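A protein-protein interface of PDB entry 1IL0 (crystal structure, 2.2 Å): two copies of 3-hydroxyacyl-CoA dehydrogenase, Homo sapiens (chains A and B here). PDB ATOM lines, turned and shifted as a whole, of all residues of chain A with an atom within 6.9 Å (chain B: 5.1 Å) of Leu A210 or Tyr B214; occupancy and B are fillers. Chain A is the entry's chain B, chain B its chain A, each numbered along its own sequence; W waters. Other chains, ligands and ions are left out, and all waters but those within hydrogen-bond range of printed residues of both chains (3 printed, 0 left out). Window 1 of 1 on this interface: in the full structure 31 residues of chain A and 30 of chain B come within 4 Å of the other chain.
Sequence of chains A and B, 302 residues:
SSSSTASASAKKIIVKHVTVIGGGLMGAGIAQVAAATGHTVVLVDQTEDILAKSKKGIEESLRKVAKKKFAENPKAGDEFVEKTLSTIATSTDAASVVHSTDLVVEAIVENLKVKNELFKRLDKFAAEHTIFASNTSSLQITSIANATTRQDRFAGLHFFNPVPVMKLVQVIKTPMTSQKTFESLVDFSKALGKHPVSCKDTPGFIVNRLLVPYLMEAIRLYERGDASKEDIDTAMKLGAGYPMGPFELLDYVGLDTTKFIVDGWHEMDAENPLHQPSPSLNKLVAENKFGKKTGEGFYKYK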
ATOM      1  N   PRO A 203      33.902  21.511 -18.766  1.00  0.00           N
ATOM      2  CA  PRO A 203      32.732  20.810 -19.305  1.00  0.00           C
ATOM      3  C   PRO A 203      32.162  21.255 -20.648  1.00  0.00           C
ATOM      4  O   PRO A 203      31.616  22.356 -20.785  1.00  0.00           O
ATOM      5  CB  PRO A 203      31.722  20.883 -18.150  1.00  0.00           C
ATOM      6  CG  PRO A 203      32.188  22.084 -17.350  1.00  0.00           C
ATOM      7  CD  PRO A 203      33.676  21.859 -17.354  1.00  0.00           C
ATOM      8  N   GLY A 204      32.280  20.353 -21.623  1.00  0.00           N
ATOM      9  CA  GLY A 204      31.812  20.591 -22.974  1.00  0.00           C
ATOM     10  C   GLY A 204      32.941  21.229 -23.750  1.00  0.00           C
ATOM     11  O   GLY A 204      32.921  21.314 -24.984  1.00  0.00           O
ATOM     12  N   PHE A 205      33.947  21.668 -23.001  1.00  0.00           N
ATOM     13  CA  PHE A 205      35.105  22.332 -23.577  1.00  0.00           C
ATOM     14  C   PHE A 205      34.568  23.633 -24.166  1.00  0.00           C
ATOM     15  O   PHE A 205      33.916  24.395 -23.448  1.00  0.00           O
ATOM     16  CB  PHE A 205      35.752  21.412 -24.626  1.00  0.00           C
ATOM     17  CG  PHE A 205      36.069  20.036 -24.090  1.00  0.00           C
ATOM     18  CD1 PHE A 205      36.849  19.885 -22.941  1.00  0.00           C
ATOM     19  CD2 PHE A 205      35.537  18.898 -24.687  1.00  0.00           C
ATOM     20  CE1 PHE A 205      37.085  18.627 -22.395  1.00  0.00           C
ATOM     21  CE2 PHE A 205      35.770  17.630 -24.145  1.00  0.00           C
ATOM     22  CZ  PHE A 205      36.543  17.498 -22.998  1.00  0.00           C
ATOM     23  N   ILE A 206      34.800  23.910 -25.443  1.00  0.00           N
ATOM     24  CA  ILE A 206      34.271  25.155 -25.991  1.00  0.00           C
ATOM     25  C   ILE A 206      32.983  24.993 -26.787  1.00  0.00           C
ATOM     26  O   ILE A 206      31.920  25.452 -26.372  1.00  0.00           O
ATOM     27  CB  ILE A 206      35.316  25.869 -26.882  1.00  0.00           C
ATOM     28  CG1 ILE A 206      36.450  26.411 -26.010  1.00  0.00           C
ATOM     29  CG2 ILE A 206      34.658  26.999 -27.663  1.00  0.00           C
ATOM     30  CD1 ILE A 206      37.548  27.112 -26.788  1.00  0.00           C
ATOM     31  N   VAL A 207      33.084  24.328 -27.929  1.00  0.00           N
ATOM     32  CA  VAL A 207      31.953  24.139 -28.816  1.00  0.00           C
ATOM     33  C   VAL A 207      30.666  23.587 -28.195  1.00  0.00           C
ATOM     34  O   VAL A 207      29.609  24.196 -28.349  1.00  0.00           O
ATOM     35  CB  VAL A 207      32.377  23.256 -30.014  1.00  0.00           C
ATOM     36  CG1 VAL A 207      31.221  23.048 -30.960  1.00  0.00           C
ATOM     37  CG2 VAL A 207      33.533  23.919 -30.748  1.00  0.00           C
ATOM     38  N   ASN A 208      30.736  22.452 -27.497  1.00  0.00           N
ATOM     39  CA  ASN A 208      29.521  21.865 -26.923  1.00  0.00           C
ATOM     40  C   ASN A 208      28.874  22.657 -25.800  1.00  0.00           C
ATOM     41  O   ASN A 208      27.652  22.638 -25.653  1.00  0.00           O
ATOM     42  CB  ASN A 208      29.768  20.428 -26.444  1.00  0.00           C
ATOM     43  CG  ASN A 208      30.152  19.508 -27.567  1.00  0.00           C
ATOM     44  OD1 ASN A 208      29.520  19.516 -28.631  1.00  0.00           O
ATOM     45  ND2 ASN A 208      31.182  18.699 -27.344  1.00  0.00           N
ATOM     46  N   ARG A 209      29.686  23.344 -25.008  1.00  0.00           N
ATOM     47  CA  ARG A 209      29.163  24.148 -23.912  1.00  0.00           C
ATOM     48  C   ARG A 209      28.268  25.283 -24.438  1.00  0.00           C
ATOM     49  O   ARG A 209      27.426  25.815 -23.710  1.00  0.00           O
ATOM     50  CB  ARG A 209      30.310  24.743 -23.105  1.00  0.00           C
ATOM     51  CG  ARG A 209      29.852  25.638 -21.966  1.00  0.00           C
ATOM     52  CD  ARG A 209      29.126  24.856 -20.892  1.00  0.00           C
ATOM     53  NE  ARG A 209      28.799  25.692 -19.742  1.00  0.00           N
ATOM     54  CZ  ARG A 209      27.845  26.618 -19.734  1.00  0.00           C
ATOM     55  NH1 ARG A 209      27.109  26.830 -20.820  1.00  0.00           N
ATOM     56  NH2 ARG A 209      27.634  27.338 -18.640  1.00  0.00           N
ATOM     57  N   LEU A 210      28.455  25.651 -25.701  1.00  0.00           N
ATOM     58  CA  LEU A 210      27.650  26.705 -26.292  1.00  0.00           C
ATOM     59  C   LEU A 210      26.626  26.119 -27.253  1.00  0.00           C
ATOM     60  O   LEU A 210      25.498  26.611 -27.346  1.00  0.00           O
ATOM     61  CB  LEU A 210      28.532  27.709 -27.042  1.00  0.00           C
ATOM     62  CG  LEU A 210      29.636  28.425 -26.263  1.00  0.00           C
ATOM     63  CD1 LEU A 210      30.345  29.396 -27.202  1.00  0.00           C
ATOM     64  CD2 LEU A 210      29.070  29.161 -25.066  1.00  0.00           C
ATOM     65  N   LEU A 211      27.014  25.065 -27.964  1.00  0.00           N
ATOM     66  CA  LEU A 211      26.126  24.447 -28.945  1.00  0.00           C
ATOM     67  C   LEU A 211      24.975  23.627 -28.352  1.00  0.00           C
ATOM     68  O   LEU A 211      23.826  23.750 -28.794  1.00  0.00           O
ATOM     69  CB  LEU A 211      26.940  23.567 -29.902  1.00  0.00           C
ATOM     70  CG  LEU A 211      26.183  22.875 -31.044  1.00  0.00           C
ATOM     71  CD1 LEU A 211      25.508  23.906 -31.948  1.00  0.00           C
ATOM     72  CD2 LEU A 211      27.158  22.035 -31.851  1.00  0.00           C
ATOM     73  N   VAL A 212      25.277  22.792 -27.360  1.00  0.00           N
ATOM     74  CA  VAL A 212      24.246  21.955 -26.758  1.00  0.00           C
ATOM     75  C   VAL A 212      23.147  22.765 -26.090  1.00  0.00           C
ATOM     76  O   VAL A 212      21.971  22.576 -26.389  1.00  0.00           O
ATOM     77  CB  VAL A 212      24.844  20.950 -25.748  1.00  0.00           C
ATOM     78  CG1 VAL A 212      23.722  20.152 -25.088  1.00  0.00           C
ATOM     79  CG2 VAL A 212      25.798  20.006 -26.466  1.00  0.00           C
ATOM     80  N   PRO A 213      23.504  23.662 -25.166  1.00  0.00           N
ATOM     81  CA  PRO A 213      22.456  24.457 -24.523  1.00  0.00           C
ATOM     82  C   PRO A 213      21.598  25.174 -25.579  1.00  0.00           C
ATOM     83  O   PRO A 213      20.393  25.373 -25.389  1.00  0.00           O
ATOM     84  CB  PRO A 213      23.262  25.416 -23.649  1.00  0.00           C
ATOM     85  CG  PRO A 213      24.426  24.553 -23.256  1.00  0.00           C
ATOM     86  CD  PRO A 213      24.817  24.032 -24.618  1.00  0.00           C
ATOM     87  N   TYR A 214      22.229  25.551 -26.690  1.00  0.00           N
ATOM     88  CA  TYR A 214      21.532  26.216 -27.782  1.00  0.00           C
ATOM     89  C   TYR A 214      20.524  25.247 -28.388  1.00  0.00           C
ATOM     90  O   TYR A 214      19.360  25.599 -28.580  1.00  0.00           O
ATOM     91  CB  TYR A 214      22.539  26.696 -28.841  1.00  0.00           C
ATOM     92  CG  TYR A 214      22.001  26.751 -30.258  1.00  0.00           C
ATOM     93  CD1 TYR A 214      20.953  27.605 -30.609  1.00  0.00           C
ATOM     94  CD2 TYR A 214      22.517  25.904 -31.246  1.00  0.00           C
ATOM     95  CE1 TYR A 214      20.427  27.606 -31.911  1.00  0.00           C
ATOM     96  CE2 TYR A 214      22.001  25.900 -32.540  1.00  0.00           C
ATOM     97  CZ  TYR A 214      20.953  26.750 -32.866  1.00  0.00           C
ATOM     98  OH  TYR A 214      20.414  26.708 -34.134  1.00  0.00           O
ATOM     99  N   LEU A 215      20.966  24.021 -28.672  1.00  0.00           N
ATOM    100  CA  LEU A 215      20.078  23.013 -29.245  1.00  0.00           C
ATOM    101  C   LEU A 215      18.934  22.664 -28.288  1.00  0.00           C
ATOM    102  O   LEU A 215      17.831  22.344 -28.723  1.00  0.00           O
ATOM    103  CB  LEU A 215      20.861  21.746 -29.599  1.00  0.00           C
ATOM    104  CG  LEU A 215      21.950  21.846 -30.671  1.00  0.00           C
ATOM    105  CD1 LEU A 215      22.640  20.487 -30.815  1.00  0.00           C
ATOM    106  CD2 LEU A 215      21.333  22.269 -32.000  1.00  0.00           C
ATOM    107  N   TYR A 242      23.290  29.398 -40.671  1.00  0.00           N
ATOM    108  CA  TYR A 242      23.640  28.069 -40.177  1.00  0.00           C
ATOM    109  C   TYR A 242      23.517  26.990 -41.244  1.00  0.00           C
ATOM    110  O   TYR A 242      22.547  26.958 -42.012  1.00  0.00           O
ATOM    111  CB  TYR A 242      22.751  27.701 -38.989  1.00  0.00           C
ATOM    112  CG  TYR A 242      23.117  28.402 -37.699  1.00  0.00           C
ATOM    113  CD1 TYR A 242      23.920  29.554 -37.696  1.00  0.00           C
ATOM    114  CD2 TYR A 242      22.656  27.925 -36.481  1.00  0.00           C
ATOM    115  CE1 TYR A 242      24.249  30.204 -36.500  1.00  0.00           C
ATOM    116  CE2 TYR A 242      22.979  28.568 -35.285  1.00  0.00           C
ATOM    117  CZ  TYR A 242      23.771  29.699 -35.301  1.00  0.00           C
ATOM    118  OH  TYR A 242      24.095  30.311 -34.110  1.00  0.00           O
ATOM    119  N   TRP A 265      25.421  16.911 -17.297  1.00  0.00           N
ATOM    120  CA  TRP A 265      25.513  18.272 -16.804  1.00  0.00           C
ATOM    121  C   TRP A 265      24.380  18.559 -15.837  1.00  0.00           C
ATOM    122  O   TRP A 265      24.577  19.276 -14.855  1.00  0.00           O
ATOM    123  CB  TRP A 265      25.486  19.276 -17.961  1.00  0.00           C
ATOM    124  CG  TRP A 265      26.697  19.188 -18.817  1.00  0.00           C
ATOM    125  CD1 TRP A 265      27.875  18.570 -18.503  1.00  0.00           C
ATOM    126  CD2 TRP A 265      26.894  19.802 -20.092  1.00  0.00           C
ATOM    127  NE1 TRP A 265      28.793  18.763 -19.500  1.00  0.00           N
ATOM    128  CE2 TRP A 265      28.221  19.517 -20.491  1.00  0.00           C
ATOM    129  CE3 TRP A 265      26.081  20.571 -20.937  1.00  0.00           C
ATOM    130  CZ2 TRP A 265      28.758  19.972 -21.702  1.00  0.00           C
ATOM    131  CZ3 TRP A 265      26.613  21.024 -22.142  1.00  0.00           C
ATOM    132  CH2 TRP A 265      27.943  20.723 -22.512  1.00  0.00           C
ATOM    133  N   LEU B 210      16.892  32.201 -29.616  1.00  0.00           N
ATOM    134  CA  LEU B 210      17.890  31.148 -29.599  1.00  0.00           C
ATOM    135  C   LEU B 210      19.313  31.682 -29.768  1.00  0.00           C
ATOM    136  O   LEU B 210      20.226  31.271 -29.052  1.00  0.00           O
ATOM    137  CB  LEU B 210      17.577  30.131 -30.697  1.00  0.00           C
ATOM    138  CG  LEU B 210      16.197  29.483 -30.548  1.00  0.00           C
ATOM    139  CD1 LEU B 210      15.939  28.513 -31.700  1.00  0.00           C
ATOM    140  CD2 LEU B 210      16.123  28.762 -29.210  1.00  0.00           C
ATOM    141  N   LEU B 211      19.488  32.613 -30.701  1.00  0.00           N
ATOM    142  CA  LEU B 211      20.796  33.190 -31.003  1.00  0.00           C
ATOM    143  C   LEU B 211      21.408  34.121 -29.941  1.00  0.00           C
ATOM    144  O   LEU B 211      22.617  34.086 -29.690  1.00  0.00           O
ATOM    145  CB  LEU B 211      20.717  33.933 -32.343  1.00  0.00           C
ATOM    146  CG  LEU B 211      22.001  34.578 -32.872  1.00  0.00           C
ATOM    147  CD1 LEU B 211      23.020  33.483 -33.179  1.00  0.00           C
ATOM    148  CD2 LEU B 211      21.697  35.379 -34.132  1.00  0.00           C
ATOM    149  N   VAL B 212      20.590  34.959 -29.320  1.00  0.00           N
ATOM    150  CA  VAL B 212      21.117  35.886 -28.324  1.00  0.00           C
ATOM    151  C   VAL B 212      21.655  35.221 -27.067  1.00  0.00           C
ATOM    152  O   VAL B 212      22.786  35.491 -26.663  1.00  0.00           O
ATOM    153  CB  VAL B 212      20.063  36.960 -27.954  1.00  0.00           C
ATOM    154  CG1 VAL B 212      20.581  37.864 -26.845  1.00  0.00           C
ATOM    155  CG2 VAL B 212      19.747  37.785 -29.182  1.00  0.00           C
ATOM    156  N   PRO B 213      20.865  34.342 -26.430  1.00  0.00           N
ATOM    157  CA  PRO B 213      21.350  33.675 -25.211  1.00  0.00           C
ATOM    158  C   PRO B 213      22.653  32.906 -25.492  1.00  0.00           C
ATOM    159  O   PRO B 213      23.517  32.772 -24.620  1.00  0.00           O
ATOM    160  CB  PRO B 213      20.180  32.771 -24.838  1.00  0.00           C
ATOM    161  CG  PRO B 213      18.981  33.573 -25.359  1.00  0.00           C
ATOM    162  CD  PRO B 213      19.500  33.890 -26.742  1.00  0.00           C
ATOM    163  N   TYR B 214      22.781  32.417 -26.722  1.00  0.00           N
ATOM    164  CA  TYR B 214      23.979  31.715 -27.166  1.00  0.00           C
ATOM    165  C   TYR B 214      25.155  32.685 -27.178  1.00  0.00           C
ATOM    166  O   TYR B 214      26.192  32.418 -26.572  1.00  0.00           O
ATOM    167  CB  TYR B 214      23.743  31.143 -28.560  1.00  0.00           C
ATOM    168  CG  TYR B 214      24.987  30.988 -29.398  1.00  0.00           C
ATOM    169  CD1 TYR B 214      25.972  30.050 -29.082  1.00  0.00           C
ATOM    170  CD2 TYR B 214      25.189  31.808 -30.506  1.00  0.00           C
ATOM    171  CE1 TYR B 214      27.133  29.942 -29.860  1.00  0.00           C
ATOM    172  CE2 TYR B 214      26.326  31.709 -31.277  1.00  0.00           C
ATOM    173  CZ  TYR B 214      27.297  30.783 -30.958  1.00  0.00           C
ATOM    174  OH  TYR B 214      28.427  30.724 -31.746  1.00  0.00           O
ATOM    175  N   LEU B 215      24.991  33.814 -27.868  1.00  0.00           N
ATOM    176  CA  LEU B 215      26.041  34.827 -27.930  1.00  0.00           C
ATOM    177  C   LEU B 215      26.396  35.264 -26.519  1.00  0.00           C
ATOM    178  O   LEU B 215      27.564  35.475 -26.211  1.00  0.00           O
ATOM    179  CB  LEU B 215      25.577  36.041 -28.734  1.00  0.00           C
ATOM    180  CG  LEU B 215      25.201  35.779 -30.191  1.00  0.00           C
ATOM    181  CD1 LEU B 215      24.555  37.028 -30.772  1.00  0.00           C
ATOM    182  CD2 LEU B 215      26.443  35.368 -30.984  1.00  0.00           C
ATOM    183  N   MET B 216      25.394  35.411 -25.656  1.00  0.00           N
ATOM    184  CA  MET B 216      25.684  35.795 -24.276  1.00  0.00           C
ATOM    185  C   MET B 216      26.447  34.673 -23.570  1.00  0.00           C
ATOM    186  O   MET B 216      27.251  34.925 -22.668  1.00  0.00           O
ATOM    187  CB  MET B 216      24.398  36.106 -23.500  1.00  0.00           C
ATOM    188  CG  MET B 216      23.678  37.373 -23.947  1.00  0.00           C
ATOM    189  SD  MET B 216      24.727  38.842 -23.818  1.00  0.00           S
ATOM    190  CE  MET B 216      25.063  38.869 -22.076  1.00  0.00           C
ATOM    191  N   GLU B 217      26.191  33.431 -23.968  1.00  0.00           N
ATOM    192  CA  GLU B 217      26.887  32.313 -23.353  1.00  0.00           C
ATOM    193  C   GLU B 217      28.345  32.337 -23.770  1.00  0.00           C
ATOM    194  O   GLU B 217      29.222  32.017 -22.976  1.00  0.00           O
ATOM    195  CB  GLU B 217      26.233  30.982 -23.733  1.00  0.00           C
ATOM    196  CG  GLU B 217      24.959  30.670 -22.936  1.00  0.00           C
ATOM    197  CD  GLU B 217      25.235  30.452 -21.448  1.00  0.00           C
ATOM    198  OE1 GLU B 217      26.014  29.535 -21.114  1.00  0.00           O
ATOM    199  OE2 GLU B 217      24.677  31.189 -20.609  1.00  0.00           O
ATOM    200  N   ALA B 218      28.608  32.721 -25.015  1.00  0.00           N
ATOM    201  CA  ALA B 218      29.986  32.807 -25.487  1.00  0.00           C
ATOM    202  C   ALA B 218      30.684  33.893 -24.680  1.00  0.00           C
ATOM    203  O   ALA B 218      31.829  33.726 -24.261  1.00  0.00           O
ATOM    204  CB  ALA B 218      30.025  33.149 -26.969  1.00  0.00           C
ATOM    205  N   ILE B 219      29.996  35.006 -24.455  1.00  0.00           N
ATOM    206  CA  ILE B 219      30.586  36.081 -23.670  1.00  0.00           C
ATOM    207  C   ILE B 219      30.900  35.581 -22.264  1.00  0.00           C
ATOM    208  O   ILE B 219      31.978  35.849 -21.734  1.00  0.00           O
ATOM    209  CB  ILE B 219      29.647  37.338 -23.588  1.00  0.00           C
ATOM    210  CG1 ILE B 219      29.501  37.979 -24.978  1.00  0.00           C
ATOM    211  CG2 ILE B 219      30.216  38.360 -22.610  1.00  0.00           C
ATOM    212  CD1 ILE B 219      28.645  39.230 -25.003  1.00  0.00           C
ATOM    213  N   LEU B 221      31.486  32.516 -21.298  1.00  0.00           N
ATOM    214  CA  LEU B 221      32.547  31.521 -21.324  1.00  0.00           C
ATOM    215  C   LEU B 221      33.899  32.229 -21.369  1.00  0.00           C
ATOM    216  O   LEU B 221      34.903  31.702 -20.882  1.00  0.00           O
ATOM    217  CB  LEU B 221      32.356  30.582 -22.527  1.00  0.00           C
ATOM    218  CG  LEU B 221      33.312  29.394 -22.662  1.00  0.00           C
ATOM    219  CD1 LEU B 221      32.743  28.395 -23.645  1.00  0.00           C
ATOM    220  CD2 LEU B 221      34.693  29.875 -23.109  1.00  0.00           C
ATOM    221  N   ILE B 232      37.430  30.783 -29.221  1.00  0.00           N
ATOM    222  CA  ILE B 232      36.015  30.499 -29.208  1.00  0.00           C
ATOM    223  C   ILE B 232      35.472  30.716 -30.631  1.00  0.00           C
ATOM    224  O   ILE B 232      34.656  29.930 -31.122  1.00  0.00           O
ATOM    225  CB  ILE B 232      35.301  31.415 -28.199  1.00  0.00           C
ATOM    226  CG1 ILE B 232      35.928  31.237 -26.812  1.00  0.00           C
ATOM    227  CG2 ILE B 232      33.832  31.077 -28.133  1.00  0.00           C
ATOM    228  CD1 ILE B 232      35.408  32.210 -25.758  1.00  0.00           C
ATOM    229  N   MET B 236      33.839  27.742 -33.029  1.00  0.00           N
ATOM    230  CA  MET B 236      32.511  27.733 -33.619  1.00  0.00           C
ATOM    231  C   MET B 236      32.534  27.677 -35.135  1.00  0.00           C
ATOM    232  O   MET B 236      31.668  27.056 -35.755  1.00  0.00           O
ATOM    233  CB  MET B 236      31.711  28.955 -33.160  1.00  0.00           C
ATOM    234  CG  MET B 236      31.507  29.044 -31.652  1.00  0.00           C
ATOM    235  SD  MET B 236      30.921  27.500 -30.888  1.00  0.00           S
ATOM    236  CE  MET B 236      29.590  27.014 -31.970  1.00  0.00           C
ATOM    237  N   TYR B 242      29.913  27.474 -38.398  1.00  0.00           N
ATOM    238  CA  TYR B 242      29.306  28.801 -38.459  1.00  0.00           C
ATOM    239  C   TYR B 242      30.125  29.766 -39.307  1.00  0.00           C
ATOM    240  O   TYR B 242      31.357  29.704 -39.330  1.00  0.00           O
ATOM    241  CB  TYR B 242      29.154  29.424 -37.067  1.00  0.00           C
ATOM    242  CG  TYR B 242      28.172  28.743 -36.147  1.00  0.00           C
ATOM    243  CD1 TYR B 242      27.306  27.760 -36.623  1.00  0.00           C
ATOM    244  CD2 TYR B 242      28.087  29.102 -34.798  1.00  0.00           C
ATOM    245  CE1 TYR B 242      26.378  27.148 -35.789  1.00  0.00           C
ATOM    246  CE2 TYR B 242      27.149  28.486 -33.949  1.00  0.00           C
ATOM    247  CZ  TYR B 242      26.301  27.514 -34.464  1.00  0.00           C
ATOM    248  OH  TYR B 242      25.331  26.932 -33.674  1.00  0.00           O
ATOM    249  N   GLY B 245      32.274  33.577 -35.872  1.00  0.00           N
ATOM    250  CA  GLY B 245      32.364  33.156 -34.488  1.00  0.00           C
ATOM    251  C   GLY B 245      31.441  34.041 -33.669  1.00  0.00           C
ATOM    252  O   GLY B 245      30.964  35.047 -34.176  1.00  0.00           O
ATOM    253  N   PRO B 246      31.176  33.707 -32.398  1.00  0.00           N
ATOM    254  CA  PRO B 246      30.291  34.483 -31.515  1.00  0.00           C
ATOM    255  C   PRO B 246      30.663  35.953 -31.321  1.00  0.00           C
ATOM    256  O   PRO B 246      29.805  36.838 -31.394  1.00  0.00           O
ATOM    257  CB  PRO B 246      30.365  33.707 -30.202  1.00  0.00           C
ATOM    258  CG  PRO B 246      30.608  32.289 -30.678  1.00  0.00           C
ATOM    259  CD  PRO B 246      31.717  32.550 -31.666  1.00  0.00           C
HETATM  260  O   HOH W   1      25.435  27.747 -23.544  1.00  0.00           O
HETATM  261  O   HOH W   2      23.971  28.683 -31.796  1.00  0.00           O
HETATM  262  O   HOH W   3      26.195  30.060 -17.979  1.00  0.00           O
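Leu A210 touches Tyr B214.
CD2 of Leu A210 touches C of Glu B217, at 3.5 Å.
CD2 of Leu A210 touches N of Ala B218 (3.6 Å).
Leu A210 touches Ile B232.
CD1 of Leu A211 touches OH of Tyr B242 (3.5 Å).
Tyr A214 touches Leu B210.
Tyr A214 touches Tyr B242.
OH of Tyr A242 touches CD1 of Leu B211, at 3.5 Å.
Tyr B214 touches Tyr A242.
Tyr A242 touches Tyr B242 (CE2 to OH, 3.3 Å).
Leu A210 touches Tyr B214, and with the chains exchanged Tyr A214 touches Leu B210.
Leu A211 touches Tyr B242, and with the chains exchanged Tyr A242 touches Leu B211.
Tyr A214 touches Tyr B242, and with the chains exchanged Tyr A242 touches Tyr B214.
Tyr B242 touches its own counterpart, Tyr A242.
Positions printed for both chains: 210, 211, 212, 213, 214, 215 and 242.
OE1 of Glu B217 is in salt-bridge range of NH1 of Arg A209, 2.9 Å away.
The backbone carbonyl oxygen (O) of Met B236 sits at hydrogen-bond distance from the backbone NH (N) of Tyr B242, at 3.2 Å.
Water W1 lies within hydrogen-bond range of O of Arg A209 and OE1 of Glu B217.
Water W2 lies within hydrogen-bond range of OH of Tyr A242 (2.8 Å) and OH of Tyr B242 (2.9 Å).
Water W3 lies within hydrogen-bond range of NH2 of Arg A209 (3.1 Å) and OE1 of Glu B217 (3.2 Å).
Printed residues of chain B within 4 Å of Leu A210: Tyr B214 (3.9 Å), Glu B217 (3.5 Å), Ala B218 (3.6 Å) and Ile B232 (3.98 Å).
Of chain A, only Leu A210 (3.9 Å) and Tyr A242 (3.9 Å) come within 4 Å of Tyr B214.
Of the printed residues of chain B, Arg A209 touches Glu B217.
Printed residues of chain A within 4 Å of Tyr B242: Leu A211, Tyr A214 and Tyr A242.
Printed residues of chain A within 4 Å of Leu B210: Tyr A214.
Of the printed residues of chain B, Leu A211 touches Tyr B242.
Printed residues of chain A within 4 Å of Glu B217: Arg A209 (2.9 Å) and Leu A210 (3.5 Å).
Ile A206 touches none of the printed residues of chain B.
The nearest printed residue of chain A that does not touch Ala B218 is Arg A209 (7.1 Å).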
